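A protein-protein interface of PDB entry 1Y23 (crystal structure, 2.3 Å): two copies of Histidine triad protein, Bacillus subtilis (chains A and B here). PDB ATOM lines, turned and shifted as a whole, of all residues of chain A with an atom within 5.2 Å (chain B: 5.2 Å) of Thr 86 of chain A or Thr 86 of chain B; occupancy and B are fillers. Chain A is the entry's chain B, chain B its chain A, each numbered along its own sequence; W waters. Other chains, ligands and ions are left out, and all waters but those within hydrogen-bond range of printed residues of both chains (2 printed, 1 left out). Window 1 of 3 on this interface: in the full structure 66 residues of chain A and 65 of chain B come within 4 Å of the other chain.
The backbone carbonyl oxygen (O) of Thr 86 of chain B is in hydrogen-bond range of the backbone NH (N) of Asn 88 of chain A (3.0 Å).
The backbone carbonyl oxygen (O) of Leu 84 of chain B lies within hydrogen-bond range of the backbone NH (N) of Asn 90 of chain A (2.8 Å).
The backbone carbonyl oxygen (O) of Thr 86 of chain A lies within hydrogen-bond range of the backbone NH (N) of Asn 88 of chain B.
The backbone carbonyl oxygen (O) of Leu 84 of chain A lies within hydrogen-bond range of the backbone NH (N) of Asn 90 of chain B (2.9 Å).
Water W2 lies within hydrogen-bond range of the side-chain hydroxyl (OH) of Tyr 101 of chain B (2.7 Å), the side-chain hydroxyl (OG1) of Thr 86 of chain A (2.9 Å) and the side-chain amide oxygen (OD1) of Asn 88 of chain B (3.0 Å).
Water W1 lies within hydrogen-bond range of the side-chain amide oxygen of Asn 88 of chain A (2.7 Å), the side-chain hydroxyl of Tyr 101 of chain A (2.7 Å) and the side-chain hydroxyl of Thr 86 of chain B (3.0 Å).
Leu 84 of chain A touches Asn 90 of chain B, and with the chains exchanged Asn 90 of chain A touches Leu 84 of chain B.
Asn 85 of chain A touches Asn 88 of chain B, and with the chains exchanged Asn 88 of chain A touches Asn 85 of chain B.
Thr 86 of chain A touches Leu 87 of chain B, and with the chains exchanged Leu 87 of chain A touches Thr 86 of chain B.
Thr 86 of chain A touches Asn 88 of chain B, and with the chains exchanged Asn 88 of chain A touches Thr 86 of chain B.
Positions printed for both chains: 53, 68, 84, 85, 86, 87, 88, 90, 101, 103, 104, 105 and 106.
Of the 9 pairs that touch across the chains among the printed residues, 9 have their exchanged pair printed and touching as well.
Hydrophobic or aromatic side chains of chain A within 4 Å of the printed part of chain B: Leu 84 and Leu 87.
Printed residues of chain B that touch a printed residue of chain A: Leu 84, Asn 85, Thr 86, Leu 87, Asn 88 and Asn 90.
Hydrophobic or aromatic side chains of chain B within 4 Å of the printed part of chain A: Leu 84 and Leu 87.
Among the printed residues, no Asp or Glu carboxylate lies within 4 Å of a Lys or Arg side-chain nitrogen of the other chain.
Val 68 of chain A touches none of the printed residues of chain B.
Printed residues of chain B within 4 Å of Asn 85 of chain A: Asn 88 (3.2 Å).
Thr 86 of chain A touches just these residues of chain B: Thr 86, Leu 87 and Asn 88.
Ile 105 of chain A touches none of the printed residues of chain B.
Printed residues of chain A within 4 Å of Asn 85 of chain B: Asn 88.
Thr 86 of chain B touches three residues of chain A.
Asn 85 of chain A touches Asn 88 of chain B (CA to O, 3.2 Å).
Thr 86 of chain A touches Thr 86 of chain B.
Leu 87 of chain B touches Thr 86 of chain A (CA to O, 3.4 Å).
CA of Leu 87 of chain A touches O of Thr 86 of chain B, at 3.4 Å.
Asn 88 of chain A touches Asn 85 of chain B (O to CA, 3.2 Å).
The backbone NH (N) of Val 53 of chain B sits at hydrogen-bond distance from the side-chain amide oxygen (OD1) of Asn 90 of chain B, 3.1 Å away.
The backbone NH of His 104 of chain B lies within hydrogen-bond range of the backbone carbonyl oxygen of Leu 87 of chain B (2.8 Å).
The side-chain amide oxygen (OD1) of Asn 88 of chain B lies within hydrogen-bond range of the side-chain amide nitrogen (ND2) of Asn 90 of chain B, at 2.9 Å.
The backbone carbonyl oxygen of Asn 85 of chain B lies within hydrogen-bond range of the backbone NH of Ile 106 of chain B.
The backbone NH of His 104 of chain A lies within hydrogen-bond range of the backbone carbonyl oxygen of Leu 87 of chain A.
The side-chain amide oxygen (OD1) of Asn 90 of chain A sits at hydrogen-bond distance from the backbone NH (N) of Val 53 of chain A (2.9 Å).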
ATOM      1  N   VAL A  53      13.529  19.642 -14.792  1.00  0.00           N
ATOM      2  CA  VAL A  53      13.523  18.231 -15.126  1.00  0.00           C
ATOM      3  C   VAL A  53      12.450  17.857 -16.156  1.00  0.00           C
ATOM      4  O   VAL A  53      12.603  16.867 -16.870  1.00  0.00           O
ATOM      5  CB  VAL A  53      13.380  17.363 -13.842  1.00  0.00           C
ATOM      6  CG1 VAL A  53      11.959  17.423 -13.299  1.00  0.00           C
ATOM      7  CG2 VAL A  53      13.789  15.948 -14.137  1.00  0.00           C
ATOM      8  N   VAL A  68      26.513  11.552 -13.628  1.00  0.00           N
ATOM      9  CA  VAL A  68      26.188  11.590 -12.204  1.00  0.00           C
ATOM     10  C   VAL A  68      26.874  10.488 -11.386  1.00  0.00           C
ATOM     11  O   VAL A  68      27.508  10.763 -10.364  1.00  0.00           O
ATOM     12  CB  VAL A  68      24.646  11.533 -11.995  1.00  0.00           C
ATOM     13  CG1 VAL A  68      24.306  11.348 -10.511  1.00  0.00           C
ATOM     14  CG2 VAL A  68      24.027  12.821 -12.512  1.00  0.00           C
ATOM     15  N   LEU A  84      25.981  10.117   0.999  1.00  0.00           N
ATOM     16  CA  LEU A  84      25.937  11.031  -0.140  1.00  0.00           C
ATOM     17  C   LEU A  84      24.525  11.129  -0.718  1.00  0.00           C
ATOM     18  O   LEU A  84      23.818  10.130  -0.813  1.00  0.00           O
ATOM     19  CB  LEU A  84      26.924  10.570  -1.226  1.00  0.00           C
ATOM     20  CG  LEU A  84      26.950  11.392  -2.521  1.00  0.00           C
ATOM     21  CD1 LEU A  84      28.347  11.423  -3.132  1.00  0.00           C
ATOM     22  CD2 LEU A  84      25.948  10.802  -3.493  1.00  0.00           C
ATOM     23  N   ASN A  85      24.104  12.336  -1.085  1.00  0.00           N
ATOM     24  CA  ASN A  85      22.774  12.509  -1.666  1.00  0.00           C
ATOM     25  C   ASN A  85      22.860  13.234  -2.998  1.00  0.00           C
ATOM     26  O   ASN A  85      23.860  13.887  -3.299  1.00  0.00           O
ATOM     27  CB  ASN A  85      21.845  13.359  -0.773  1.00  0.00           C
ATOM     28  CG  ASN A  85      21.948  13.031   0.705  1.00  0.00           C
ATOM     29  OD1 ASN A  85      22.818  13.547   1.403  1.00  0.00           O
ATOM     30  ND2 ASN A  85      21.049  12.182   1.191  1.00  0.00           N
ATOM     31  N   THR A  86      21.810  13.090  -3.799  1.00  0.00           N
ATOM     32  CA  THR A  86      21.700  13.825  -5.052  1.00  0.00           C
ATOM     33  C   THR A  86      20.331  14.471  -4.897  1.00  0.00           C
ATOM     34  O   THR A  86      19.372  13.831  -4.455  1.00  0.00           O
ATOM     35  CB  THR A  86      21.762  12.919  -6.348  1.00  0.00           C
ATOM     36  OG1 THR A  86      20.599  12.081  -6.441  1.00  0.00           O
ATOM     37  CG2 THR A  86      23.023  12.062  -6.343  1.00  0.00           C
ATOM     38  N   LEU A  87      20.276  15.760  -5.217  1.00  0.00           N
ATOM     39  CA  LEU A  87      19.065  16.558  -5.101  1.00  0.00           C
ATOM     40  C   LEU A  87      18.863  17.476  -6.290  1.00  0.00           C
ATOM     41  O   LEU A  87      19.780  18.164  -6.739  1.00  0.00           O
ATOM     42  CB  LEU A  87      19.116  17.413  -3.834  1.00  0.00           C
ATOM     43  CG  LEU A  87      17.962  18.392  -3.592  1.00  0.00           C
ATOM     44  CD1 LEU A  87      16.671  17.625  -3.331  1.00  0.00           C
ATOM     45  CD2 LEU A  87      18.299  19.288  -2.402  1.00  0.00           C
ATOM     46  N   ASN A  88      17.637  17.489  -6.783  1.00  0.00           N
ATOM     47  CA  ASN A  88      17.268  18.316  -7.911  1.00  0.00           C
ATOM     48  C   ASN A  88      16.034  19.109  -7.477  1.00  0.00           C
ATOM     49  O   ASN A  88      15.086  18.529  -6.956  1.00  0.00           O
ATOM     50  CB  ASN A  88      16.927  17.415  -9.091  1.00  0.00           C
ATOM     51  CG  ASN A  88      16.245  18.156 -10.206  1.00  0.00           C
ATOM     52  OD1 ASN A  88      15.358  17.625 -10.870  1.00  0.00           O
ATOM     53  ND2 ASN A  88      16.658  19.387 -10.428  1.00  0.00           N
ATOM     54  N   ASN A  90      12.936  21.791  -8.616  1.00  0.00           N
ATOM     55  CA  ASN A  90      12.198  22.330  -9.749  1.00  0.00           C
ATOM     56  C   ASN A  90      11.112  23.286  -9.272  1.00  0.00           C
ATOM     57  O   ASN A  90      10.087  22.867  -8.730  1.00  0.00           O
ATOM     58  CB  ASN A  90      11.584  21.184 -10.546  1.00  0.00           C
ATOM     59  CG  ASN A  90      12.627  20.187 -11.016  1.00  0.00           C
ATOM     60  OD1 ASN A  90      13.338  20.423 -11.992  1.00  0.00           O
ATOM     61  ND2 ASN A  90      12.736  19.075 -10.307  1.00  0.00           N
ATOM     62  N   TYR A 101      18.321  23.567 -15.247  1.00  0.00           N
ATOM     63  CA  TYR A 101      18.393  22.276 -14.561  1.00  0.00           C
ATOM     64  C   TYR A 101      19.768  21.996 -13.978  1.00  0.00           C
ATOM     65  O   TYR A 101      20.784  22.155 -14.653  1.00  0.00           O
ATOM     66  CB  TYR A 101      18.009  21.121 -15.505  1.00  0.00           C
ATOM     67  CG  TYR A 101      18.042  19.753 -14.840  1.00  0.00           C
ATOM     68  CD1 TYR A 101      16.933  19.268 -14.133  1.00  0.00           C
ATOM     69  CD2 TYR A 101      19.207  18.978 -14.853  1.00  0.00           C
ATOM     70  CE1 TYR A 101      16.989  18.048 -13.451  1.00  0.00           C
ATOM     71  CE2 TYR A 101      19.278  17.761 -14.176  1.00  0.00           C
ATOM     72  CZ  TYR A 101      18.167  17.299 -13.473  1.00  0.00           C
ATOM     73  OH  TYR A 101      18.235  16.106 -12.781  1.00  0.00           O
ATOM     74  N   MET A 103      21.746  19.312 -10.783  1.00  0.00           N
ATOM     75  CA  MET A 103      21.667  18.255  -9.790  1.00  0.00           C
ATOM     76  C   MET A 103      22.731  18.523  -8.737  1.00  0.00           C
ATOM     77  O   MET A 103      23.879  18.804  -9.077  1.00  0.00           O
ATOM     78  CB  MET A 103      21.942  16.903 -10.448  1.00  0.00           C
ATOM     79  CG  MET A 103      21.948  15.727  -9.491  1.00  0.00           C
ATOM     80  SD  MET A 103      20.303  15.028  -9.240  1.00  0.00           S
ATOM     81  CE  MET A 103      20.398  13.583 -10.297  1.00  0.00           C
ATOM     82  N   HIS A 104      22.348  18.467  -7.464  1.00  0.00           N
ATOM     83  CA  HIS A 104      23.307  18.661  -6.381  1.00  0.00           C
ATOM     84  C   HIS A 104      23.844  17.299  -5.975  1.00  0.00           C
ATOM     85  O   HIS A 104      23.075  16.353  -5.789  1.00  0.00           O
ATOM     86  CB  HIS A 104      22.661  19.255  -5.125  1.00  0.00           C
ATOM     87  CG  HIS A 104      22.186  20.661  -5.273  1.00  0.00           C
ATOM     88  ND1 HIS A 104      20.893  20.976  -5.637  1.00  0.00           N
ATOM     89  CD2 HIS A 104      22.811  21.842  -5.053  1.00  0.00           C
ATOM     90  CE1 HIS A 104      20.743  22.289  -5.627  1.00  0.00           C
ATOM     91  NE2 HIS A 104      21.892  22.837  -5.276  1.00  0.00           N
ATOM     92  N   ILE A 105      25.158  17.203  -5.840  1.00  0.00           N
ATOM     93  CA  ILE A 105      25.785  15.972  -5.388  1.00  0.00           C
ATOM     94  C   ILE A 105      26.364  16.340  -4.032  1.00  0.00           C
ATOM     95  O   ILE A 105      27.406  16.991  -3.941  1.00  0.00           O
ATOM     96  CB  ILE A 105      26.900  15.519  -6.344  1.00  0.00           C
ATOM     97  CG1 ILE A 105      26.279  15.167  -7.703  1.00  0.00           C
ATOM     98  CG2 ILE A 105      27.640  14.325  -5.756  1.00  0.00           C
ATOM     99  CD1 ILE A 105      27.251  14.580  -8.695  1.00  0.00           C
ATOM    100  N   ILE A 106      25.675  15.933  -2.974  1.00  0.00           N
ATOM    101  CA  ILE A 106      26.100  16.289  -1.631  1.00  0.00           C
ATOM    102  C   ILE A 106      26.694  15.163  -0.803  1.00  0.00           C
ATOM    103  O   ILE A 106      26.001  14.239  -0.392  1.00  0.00           O
ATOM    104  CB  ILE A 106      24.928  16.921  -0.856  1.00  0.00           C
ATOM    105  CG1 ILE A 106      24.347  18.090  -1.672  1.00  0.00           C
ATOM    106  CG2 ILE A 106      25.405  17.413   0.501  1.00  0.00           C
ATOM    107  CD1 ILE A 106      22.960  18.534  -1.234  1.00  0.00           C
ATOM    108  N   VAL B  53      23.838   4.527  -6.125  1.00  0.00           N
ATOM    109  CA  VAL B  53      24.244   5.253  -7.321  1.00  0.00           C
ATOM    110  C   VAL B  53      25.668   4.917  -7.785  1.00  0.00           C
ATOM    111  O   VAL B  53      26.014   5.157  -8.943  1.00  0.00           O
ATOM    112  CB  VAL B  53      24.122   6.788  -7.083  1.00  0.00           C
ATOM    113  CG1 VAL B  53      25.183   7.250  -6.097  1.00  0.00           C
ATOM    114  CG2 VAL B  53      24.243   7.552  -8.401  1.00  0.00           C
ATOM    115  N   VAL B  68      12.553   9.233 -15.169  1.00  0.00           N
ATOM    116  CA  VAL B  68      12.347  10.267 -14.163  1.00  0.00           C
ATOM    117  C   VAL B  68      11.647  11.505 -14.726  1.00  0.00           C
ATOM    118  O   VAL B  68      10.694  12.003 -14.124  1.00  0.00           O
ATOM    119  CB  VAL B  68      13.699  10.674 -13.499  1.00  0.00           C
ATOM    120  CG1 VAL B  68      13.507  11.872 -12.585  1.00  0.00           C
ATOM    121  CG2 VAL B  68      14.256   9.491 -12.702  1.00  0.00           C
ATOM    122  N   LEU B  84       8.644  20.636  -7.300  1.00  0.00           N
ATOM    123  CA  LEU B  84       8.951  19.207  -7.303  1.00  0.00           C
ATOM    124  C   LEU B  84      10.440  18.970  -7.128  1.00  0.00           C
ATOM    125  O   LEU B  84      11.258  19.677  -7.714  1.00  0.00           O
ATOM    126  CB  LEU B  84       8.484  18.559  -8.616  1.00  0.00           C
ATOM    127  CG  LEU B  84       8.669  17.051  -8.800  1.00  0.00           C
ATOM    128  CD1 LEU B  84       7.514  16.507  -9.629  1.00  0.00           C
ATOM    129  CD2 LEU B  84      10.006  16.731  -9.472  1.00  0.00           C
ATOM    130  N   ASN B  85      10.781  17.975  -6.316  1.00  0.00           N
ATOM    131  CA  ASN B  85      12.173  17.624  -6.070  1.00  0.00           C
ATOM    132  C   ASN B  85      12.399  16.154  -6.411  1.00  0.00           C
ATOM    133  O   ASN B  85      11.451  15.375  -6.520  1.00  0.00           O
ATOM    134  CB  ASN B  85      12.560  17.810  -4.587  1.00  0.00           C
ATOM    135  CG  ASN B  85      12.186  19.180  -4.028  1.00  0.00           C
ATOM    136  OD1 ASN B  85      11.169  19.324  -3.352  1.00  0.00           O
ATOM    137  ND2 ASN B  85      13.009  20.186  -4.305  1.00  0.00           N
ATOM    138  N   THR B  86      13.667  15.799  -6.607  1.00  0.00           N
ATOM    139  CA  THR B  86      14.070  14.415  -6.834  1.00  0.00           C
ATOM    140  C   THR B  86      15.211  14.242  -5.839  1.00  0.00           C
ATOM    141  O   THR B  86      16.130  15.069  -5.781  1.00  0.00           O
ATOM    142  CB  THR B  86      14.576  14.113  -8.285  1.00  0.00           C
ATOM    143  OG1 THR B  86      15.870  14.690  -8.486  1.00  0.00           O
ATOM    144  CG2 THR B  86      13.603  14.646  -9.314  1.00  0.00           C
ATOM    145  N   LEU B  87      15.136  13.178  -5.043  1.00  0.00           N
ATOM    146  CA  LEU B  87      16.137  12.911  -4.015  1.00  0.00           C
ATOM    147  C   LEU B  87      16.579  11.463  -4.001  1.00  0.00           C
ATOM    148  O   LEU B  87      15.757  10.544  -4.030  1.00  0.00           O
ATOM    149  CB  LEU B  87      15.576  13.286  -2.637  1.00  0.00           C
ATOM    150  CG  LEU B  87      16.409  12.988  -1.392  1.00  0.00           C
ATOM    151  CD1 LEU B  87      17.551  13.986  -1.254  1.00  0.00           C
ATOM    152  CD2 LEU B  87      15.504  13.044  -0.175  1.00  0.00           C
ATOM    153  N   ASN B  88      17.893  11.280  -3.966  1.00  0.00           N
ATOM    154  CA  ASN B  88      18.515   9.962  -3.922  1.00  0.00           C
ATOM    155  C   ASN B  88      19.374   9.925  -2.668  1.00  0.00           C
ATOM    156  O   ASN B  88      20.128  10.863  -2.403  1.00  0.00           O
ATOM    157  CB  ASN B  88      19.408   9.740  -5.144  1.00  0.00           C
ATOM    158  CG  ASN B  88      20.244   8.476  -5.034  1.00  0.00           C
ATOM    159  OD1 ASN B  88      21.409   8.455  -5.426  1.00  0.00           O
ATOM    160  ND2 ASN B  88      19.644   7.413  -4.508  1.00  0.00           N
ATOM    161  N   ASN B  90      22.253   7.769  -0.456  1.00  0.00           N
ATOM    162  CA  ASN B  90      23.265   6.721  -0.491  1.00  0.00           C
ATOM    163  C   ASN B  90      23.975   6.631   0.838  1.00  0.00           C
ATOM    164  O   ASN B  90      24.754   7.514   1.194  1.00  0.00           O
ATOM    165  CB  ASN B  90      24.280   6.999  -1.587  1.00  0.00           C
ATOM    166  CG  ASN B  90      23.640   7.073  -2.944  1.00  0.00           C
ATOM    167  OD1 ASN B  90      23.280   6.054  -3.537  1.00  0.00           O
ATOM    168  ND2 ASN B  90      23.467   8.295  -3.441  1.00  0.00           N
ATOM    169  N   TYR B 101      19.138   1.111  -5.126  1.00  0.00           N
ATOM    170  CA  TYR B 101      19.040   2.446  -5.697  1.00  0.00           C
ATOM    171  C   TYR B 101      17.600   2.855  -6.000  1.00  0.00           C
ATOM    172  O   TYR B 101      16.819   2.072  -6.542  1.00  0.00           O
ATOM    173  CB  TYR B 101      19.861   2.563  -6.980  1.00  0.00           C
ATOM    174  CG  TYR B 101      19.826   3.975  -7.533  1.00  0.00           C
ATOM    175  CD1 TYR B 101      20.779   4.926  -7.144  1.00  0.00           C
ATOM    176  CD2 TYR B 101      18.791   4.386  -8.377  1.00  0.00           C
ATOM    177  CE1 TYR B 101      20.695   6.251  -7.581  1.00  0.00           C
ATOM    178  CE2 TYR B 101      18.699   5.703  -8.811  1.00  0.00           C
ATOM    179  CZ  TYR B 101      19.647   6.627  -8.412  1.00  0.00           C
ATOM    180  OH  TYR B 101      19.530   7.924  -8.831  1.00  0.00           O
ATOM    181  N   MET B 103      14.996   6.698  -6.693  1.00  0.00           N
ATOM    182  CA  MET B 103      14.866   8.141  -6.814  1.00  0.00           C
ATOM    183  C   MET B 103      13.513   8.562  -6.249  1.00  0.00           C
ATOM    184  O   MET B 103      12.460   8.070  -6.673  1.00  0.00           O
ATOM    185  CB  MET B 103      14.967   8.557  -8.284  1.00  0.00           C
ATOM    186  CG  MET B 103      14.967  10.061  -8.520  1.00  0.00           C
ATOM    187  SD  MET B 103      16.499  10.867  -7.996  1.00  0.00           S
ATOM    188  CE  MET B 103      17.510  10.642  -9.480  1.00  0.00           C
ATOM    189  N   HIS B 104      13.546   9.455  -5.269  1.00  0.00           N
ATOM    190  CA  HIS B 104      12.316   9.959  -4.682  1.00  0.00           C
ATOM    191  C   HIS B 104      11.831  11.100  -5.567  1.00  0.00           C
ATOM    192  O   HIS B 104      12.578  12.034  -5.815  1.00  0.00           O
ATOM    193  CB  HIS B 104      12.550  10.534  -3.276  1.00  0.00           C
ATOM    194  CG  HIS B 104      12.701   9.507  -2.197  1.00  0.00           C
ATOM    195  ND1 HIS B 104      13.931   9.074  -1.746  1.00  0.00           N
ATOM    196  CD2 HIS B 104      11.777   8.859  -1.449  1.00  0.00           C
ATOM    197  CE1 HIS B 104      13.754   8.206  -0.765  1.00  0.00           C
ATOM    198  NE2 HIS B 104      12.457   8.058  -0.566  1.00  0.00           N
ATOM    199  N   ILE B 105      10.612  11.013  -6.086  1.00  0.00           N
ATOM    200  CA  ILE B 105      10.080  12.126  -6.859  1.00  0.00           C
ATOM    201  C   ILE B 105       9.028  12.695  -5.913  1.00  0.00           C
ATOM    202  O   ILE B 105       8.008  12.055  -5.637  1.00  0.00           O
ATOM    203  CB  ILE B 105       9.445  11.693  -8.194  1.00  0.00           C
ATOM    204  CG1 ILE B 105      10.537  11.194  -9.154  1.00  0.00           C
ATOM    205  CG2 ILE B 105       8.729  12.886  -8.837  1.00  0.00           C
ATOM    206  CD1 ILE B 105      10.021  10.779 -10.535  1.00  0.00           C
ATOM    207  N   ILE B 106       9.305  13.887  -5.394  1.00  0.00           N
ATOM    208  CA  ILE B 106       8.430  14.529  -4.419  1.00  0.00           C
ATOM    209  C   ILE B 106       7.767  15.819  -4.862  1.00  0.00           C
ATOM    210  O   ILE B 106       8.420  16.860  -4.974  1.00  0.00           O
ATOM    211  CB  ILE B 106       9.201  14.838  -3.119  1.00  0.00           C
ATOM    212  CG1 ILE B 106       9.838  13.554  -2.574  1.00  0.00           C
ATOM    213  CG2 ILE B 106       8.266  15.453  -2.090  1.00  0.00           C
ATOM    214  CD1 ILE B 106      10.905  13.800  -1.528  1.00  0.00           C
HETATM  215  O   HOH W   1      16.117  15.088 -11.405  1.00  0.00           O
HETATM  216  O   HOH W   2      21.304   9.792  -8.127  1.00  0.00           O
